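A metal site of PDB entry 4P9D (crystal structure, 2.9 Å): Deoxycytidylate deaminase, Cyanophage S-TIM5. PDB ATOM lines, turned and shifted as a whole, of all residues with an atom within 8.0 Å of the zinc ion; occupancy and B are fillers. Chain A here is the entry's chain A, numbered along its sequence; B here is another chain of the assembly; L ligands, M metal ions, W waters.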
ATOM      1  N   VAL A  30      23.458 -20.381 -17.310  1.00  0.00           N
ATOM      2  CA  VAL A  30      23.512 -19.878 -18.669  1.00  0.00           C
ATOM      3  C   VAL A  30      24.943 -19.572 -19.105  1.00  0.00           C
ATOM      4  O   VAL A  30      25.750 -19.076 -18.304  1.00  0.00           O
ATOM      5  CB  VAL A  30      22.656 -18.606 -18.834  1.00  0.00           C
ATOM      6  CG1 VAL A  30      22.400 -18.309 -20.302  1.00  0.00           C
ATOM      7  CG2 VAL A  30      21.341 -18.772 -18.104  1.00  0.00           C
ATOM      8  N   LEU A  69      24.955 -11.088 -12.595  1.00  0.00           N
ATOM      9  CA  LEU A  69      25.009 -10.669 -13.987  1.00  0.00           C
ATOM     10  C   LEU A  69      24.483 -11.776 -14.872  1.00  0.00           C
ATOM     11  O   LEU A  69      24.712 -12.959 -14.601  1.00  0.00           O
ATOM     12  CB  LEU A  69      26.432 -10.290 -14.384  1.00  0.00           C
ATOM     13  CG  LEU A  69      27.060  -9.094 -13.663  1.00  0.00           C
ATOM     14  CD1 LEU A  69      28.536  -9.358 -13.399  1.00  0.00           C
ATOM     15  CD2 LEU A  69      26.886  -7.832 -14.479  1.00  0.00           C
ATOM     16  N   HIS A  70      23.775 -11.415 -15.935  1.00  0.00           N
ATOM     17  CA  HIS A  70      23.365 -12.397 -16.929  1.00  0.00           C
ATOM     18  C   HIS A  70      24.598 -12.822 -17.725  1.00  0.00           C
ATOM     19  O   HIS A  70      25.570 -12.074 -17.829  1.00  0.00           O
ATOM     20  CB  HIS A  70      22.290 -11.843 -17.850  1.00  0.00           C
ATOM     21  CG  HIS A  70      20.933 -11.759 -17.214  1.00  0.00           C
ATOM     22  ND1 HIS A  70      19.808 -11.351 -17.898  1.00  0.00           N
ATOM     23  CD2 HIS A  70      20.521 -12.049 -15.956  1.00  0.00           C
ATOM     24  CE1 HIS A  70      18.770 -11.378 -17.089  1.00  0.00           C
ATOM     25  NE2 HIS A  70      19.170 -11.805 -15.909  1.00  0.00           N
ATOM     26  N   ALA A  71      24.543 -14.030 -18.288  1.00  0.00           N
ATOM     27  CA  ALA A  71      25.638 -14.543 -19.104  1.00  0.00           C
ATOM     28  C   ALA A  71      25.913 -13.604 -20.275  1.00  0.00           C
ATOM     29  O   ALA A  71      27.062 -13.386 -20.660  1.00  0.00           O
ATOM     30  CB  ALA A  71      25.312 -15.937 -19.608  1.00  0.00           C
ATOM     31  N   GLU A  72      24.844 -13.047 -20.828  1.00  0.00           N
ATOM     32  CA  GLU A  72      24.933 -12.125 -21.949  1.00  0.00           C
ATOM     33  C   GLU A  72      25.536 -10.795 -21.505  1.00  0.00           C
ATOM     34  O   GLU A  72      26.232 -10.135 -22.259  1.00  0.00           O
ATOM     35  CB  GLU A  72      23.559 -11.901 -22.574  1.00  0.00           C
ATOM     36  CG  GLU A  72      22.907 -13.160 -23.172  1.00  0.00           C
ATOM     37  CD  GLU A  72      22.442 -14.140 -22.115  1.00  0.00           C
ATOM     38  OE1 GLU A  72      22.045 -13.694 -21.016  1.00  0.00           O
ATOM     39  OE2 GLU A  72      22.471 -15.362 -22.381  1.00  0.00           O
ATOM     40  N   GLN A  73      25.250 -10.415 -20.261  1.00  0.00           N
ATOM     41  CA  GLN A  73      25.787  -9.172 -19.693  1.00  0.00           C
ATOM     42  C   GLN A  73      27.297  -9.268 -19.514  1.00  0.00           C
ATOM     43  O   GLN A  73      28.029  -8.349 -19.896  1.00  0.00           O
ATOM     44  CB  GLN A  73      25.114  -8.859 -18.359  1.00  0.00           C
ATOM     45  CG  GLN A  73      23.953  -7.878 -18.456  1.00  0.00           C
ATOM     46  CD  GLN A  73      23.278  -7.665 -17.118  1.00  0.00           C
ATOM     47  OE1 GLN A  73      23.121  -8.594 -16.333  1.00  0.00           O
ATOM     48  NE2 GLN A  73      22.864  -6.427 -16.855  1.00  0.00           N
ATOM     49  N   HIS A  95      20.747 -20.326 -23.412  1.00  0.00           N
ATOM     50  CA  HIS A  95      19.338 -19.962 -23.308  1.00  0.00           C
ATOM     51  C   HIS A  95      19.081 -18.629 -24.014  1.00  0.00           C
ATOM     52  O   HIS A  95      19.961 -17.776 -24.066  1.00  0.00           O
ATOM     53  CB  HIS A  95      18.914 -19.851 -21.844  1.00  0.00           C
ATOM     54  CG  HIS A  95      19.245 -21.075 -21.021  1.00  0.00           C
ATOM     55  ND1 HIS A  95      20.537 -21.426 -20.710  1.00  0.00           N
ATOM     56  CD2 HIS A  95      18.448 -22.005 -20.460  1.00  0.00           C
ATOM     57  CE1 HIS A  95      20.526 -22.536 -19.993  1.00  0.00           C
ATOM     58  NE2 HIS A  95      19.273 -22.906 -19.815  1.00  0.00           N
ATOM     59  N   SER A  96      17.872 -18.469 -24.542  1.00  0.00           N
ATOM     60  CA  SER A  96      17.490 -17.226 -25.196  1.00  0.00           C
ATOM     61  C   SER A  96      17.564 -16.051 -24.221  1.00  0.00           C
ATOM     62  O   SER A  96      17.061 -16.141 -23.093  1.00  0.00           O
ATOM     63  CB  SER A  96      16.083 -17.346 -25.777  1.00  0.00           C
ATOM     64  OG  SER A  96      15.118 -17.528 -24.756  1.00  0.00           O
ATOM     65  N   PRO A  97      18.193 -14.946 -24.646  1.00  0.00           N
ATOM     66  CA  PRO A  97      18.467 -13.799 -23.788  1.00  0.00           C
ATOM     67  C   PRO A  97      17.220 -12.989 -23.412  1.00  0.00           C
ATOM     68  O   PRO A  97      16.211 -13.043 -24.109  1.00  0.00           O
ATOM     69  CB  PRO A  97      19.421 -12.956 -24.628  1.00  0.00           C
ATOM     70  CG  PRO A  97      19.050 -13.273 -26.030  1.00  0.00           C
ATOM     71  CD  PRO A  97      18.684 -14.728 -26.022  1.00  0.00           C
ATOM     72  N   CYS A  98      17.313 -12.254 -22.304  1.00  0.00           N
ATOM     73  CA  CYS A  98      16.225 -11.415 -21.809  1.00  0.00           C
ATOM     74  C   CYS A  98      16.139 -10.135 -22.648  1.00  0.00           C
ATOM     75  O   CYS A  98      17.089  -9.807 -23.367  1.00  0.00           O
ATOM     76  CB  CYS A  98      16.433 -11.090 -20.328  1.00  0.00           C
ATOM     77  SG  CYS A  98      17.732  -9.873 -20.009  1.00  0.00           S
ATOM     78  N   PRO A  99      15.009  -9.407 -22.565  1.00  0.00           N
ATOM     79  CA  PRO A  99      14.847  -8.170 -23.338  1.00  0.00           C
ATOM     80  C   PRO A  99      15.935  -7.117 -23.105  1.00  0.00           C
ATOM     81  O   PRO A  99      16.348  -6.467 -24.067  1.00  0.00           O
ATOM     82  CB  PRO A  99      13.489  -7.645 -22.844  1.00  0.00           C
ATOM     83  CG  PRO A  99      12.740  -8.849 -22.469  1.00  0.00           C
ATOM     84  CD  PRO A  99      13.752  -9.816 -21.908  1.00  0.00           C
ATOM     85  N   ASP A 100      16.388  -6.937 -21.871  1.00  0.00           N
ATOM     86  CA  ASP A 100      17.380  -5.908 -21.564  1.00  0.00           C
ATOM     87  C   ASP A 100      18.707  -6.172 -22.261  1.00  0.00           C
ATOM     88  O   ASP A 100      19.267  -5.296 -22.900  1.00  0.00           O
ATOM     89  CB  ASP A 100      17.594  -5.792 -20.056  1.00  0.00           C
ATOM     90  CG  ASP A 100      18.440  -4.591 -19.680  1.00  0.00           C
ATOM     91  OD1 ASP A 100      18.113  -3.466 -20.130  1.00  0.00           O
ATOM     92  OD2 ASP A 100      19.427  -4.769 -18.950  1.00  0.00           O
ATOM     93  N   CYS A 101      19.207  -7.397 -22.129  1.00  0.00           N
ATOM     94  CA  CYS A 101      20.429  -7.802 -22.809  1.00  0.00           C
ATOM     95  C   CYS A 101      20.236  -7.745 -24.319  1.00  0.00           C
ATOM     96  O   CYS A 101      21.152  -7.392 -25.059  1.00  0.00           O
ATOM     97  CB  CYS A 101      20.856  -9.211 -22.379  1.00  0.00           C
ATOM     98  SG  CYS A 101      21.160  -9.404 -20.601  1.00  0.00           S
ATOM     99  N   SER A 102      19.031  -8.092 -24.754  1.00  0.00           N
ATOM    100  CA  SER A 102      18.675  -8.095 -26.174  1.00  0.00           C
ATOM    101  C   SER A 102      18.756  -6.694 -26.776  1.00  0.00           C
ATOM    102  O   SER A 102      19.120  -6.533 -27.946  1.00  0.00           O
ATOM    103  CB  SER A 102      17.280  -8.665 -26.370  1.00  0.00           C
ATOM    104  OG  SER A 102      17.235 -10.046 -26.048  1.00  0.00           O
ATOM    105  N   MET A 104      20.861  -4.338 -25.794  1.00  0.00           N
ATOM    106  CA  MET A 104      22.282  -4.013 -25.890  1.00  0.00           C
ATOM    107  C   MET A 104      22.996  -4.872 -26.929  1.00  0.00           C
ATOM    108  O   MET A 104      23.971  -4.441 -27.541  1.00  0.00           O
ATOM    109  CB  MET A 104      22.942  -4.181 -24.516  1.00  0.00           C
ATOM    110  CG  MET A 104      22.554  -3.107 -23.512  1.00  0.00           C
ATOM    111  SD  MET A 104      23.228  -3.431 -21.864  1.00  0.00           S
ATOM    112  CE  MET A 104      22.192  -4.796 -21.347  1.00  0.00           C
ATOM    113  N   ILE A 105      22.504  -6.096 -27.117  1.00  0.00           N
ATOM    114  CA  ILE A 105      23.075  -7.008 -28.112  1.00  0.00           C
ATOM    115  C   ILE A 105      22.902  -6.443 -29.513  1.00  0.00           C
ATOM    116  O   ILE A 105      23.831  -6.449 -30.320  1.00  0.00           O
ATOM    117  CB  ILE A 105      22.443  -8.415 -28.024  1.00  0.00           C
ATOM    118  CG1 ILE A 105      23.138  -9.264 -26.963  1.00  0.00           C
ATOM    119  CG2 ILE A 105      22.536  -9.128 -29.362  1.00  0.00           C
ATOM    120  CD1 ILE A 105      22.210 -10.180 -26.192  1.00  0.00           C
ATOM    121  N   ASP B 100      21.263  -1.535 -12.348  1.00  0.00           N
ATOM    122  CA  ASP B 100      21.771  -2.480 -13.296  1.00  0.00           C
ATOM    123  C   ASP B 100      22.917  -1.944 -14.086  1.00  0.00           C
ATOM    124  O   ASP B 100      23.853  -2.629 -14.348  1.00  0.00           O
ATOM    125  CB  ASP B 100      20.725  -2.975 -14.237  1.00  0.00           C
ATOM    126  CG  ASP B 100      21.282  -3.958 -15.226  1.00  0.00           C
ATOM    127  OD1 ASP B 100      22.441  -4.295 -15.042  1.00  0.00           O
ATOM    128  OD2 ASP B 100      20.642  -4.387 -16.175  1.00  0.00           O
HETATM  129  P1  LIG L   1      15.706 -15.791 -12.757  1.00  0.00           P
HETATM  130  O1  LIG L   1      15.955 -15.868 -11.317  1.00  0.00           O
HETATM  131  O2  LIG L   1      15.633 -14.412 -13.291  1.00  0.00           O
HETATM  132  O3  LIG L   1      14.673 -16.702 -13.285  1.00  0.00           O
HETATM  133  O4  LIG L   1      17.050 -16.312 -13.413  1.00  0.00           O
HETATM  134  C1  LIG L   1      17.824 -17.316 -12.729  1.00  0.00           C
HETATM  135  C2  LIG L   1      19.288 -17.351 -13.189  1.00  0.00           C
HETATM  136  O5  LIG L   1      19.336 -17.271 -14.641  1.00  0.00           O
HETATM  137  C3  LIG L   1      20.061 -16.130 -12.712  1.00  0.00           C
HETATM  138  O6  LIG L   1      21.467 -16.424 -12.701  1.00  0.00           O
HETATM  139  C4  LIG L   1      19.815 -15.188 -13.850  1.00  0.00           C
HETATM  140  C5  LIG L   1      20.199 -16.159 -14.935  1.00  0.00           C
HETATM  141  N1  LIG L   1      19.874 -15.647 -16.288  1.00  0.00           N
HETATM  142  C6  LIG L   1      20.838 -15.446 -17.198  1.00  0.00           C
HETATM  143  O7  LIG L   1      22.017 -15.671 -16.916  1.00  0.00           O
HETATM  144  N2  LIG L   1      20.522 -14.968 -18.472  1.00  0.00           N
HETATM  145  C7  LIG L   1      19.188 -14.694 -18.808  1.00  0.00           C
HETATM  146  O8  LIG L   1      18.906 -14.269 -19.933  1.00  0.00           O
HETATM  147  C8  LIG L   1      18.199 -14.905 -17.862  1.00  0.00           C
HETATM  148  C9  LIG L   1      16.868 -14.650 -18.174  1.00  0.00           C
HETATM  149  C10 LIG L   1      18.542 -15.382 -16.601  1.00  0.00           C
HETATM  150 ZN    ZN M   1      19.677 -10.985 -19.888  1.00  0.00          ZN
HETATM  151  O   HOH W   1      19.967 -12.637 -21.120  1.00  0.00           O
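An oxygen (O8) of the ligand lies within hydrogen-bond range of the backbone NH (N) of Cys 98 (3.5 Å). The side-chain carboxylate (OE1) of Glu 72 lies within hydrogen-bond range of a nitrogen (N2) of the ligand, at 3.2 Å. N of Ala 71 lies within hydrogen-bond range of O7 of the ligand (3.3 Å).
The backbone NH (N) of His 70 sits at hydrogen-bond distance from the side-chain amide oxygen (OE1) of Gln 73 (2.9 Å). The side-chain sulfur (SG) of Cys 98 lies close to the backbone NH (N) of Asp 100 of chain A, 3.7 Å away. The backbone carbonyl oxygen of Cys 98 lies within hydrogen-bond range of the side-chain hydroxyl of Ser 102 (2.7 Å).
Glu 72 touches the zinc ion (OE1 to ZN, 3.8 Å).
The zinc ion is bound by a ring nitrogen (ND1) of His 70, water W1, the side-chain sulfur of Cys 98 and the side-chain sulfur of Cys 101.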
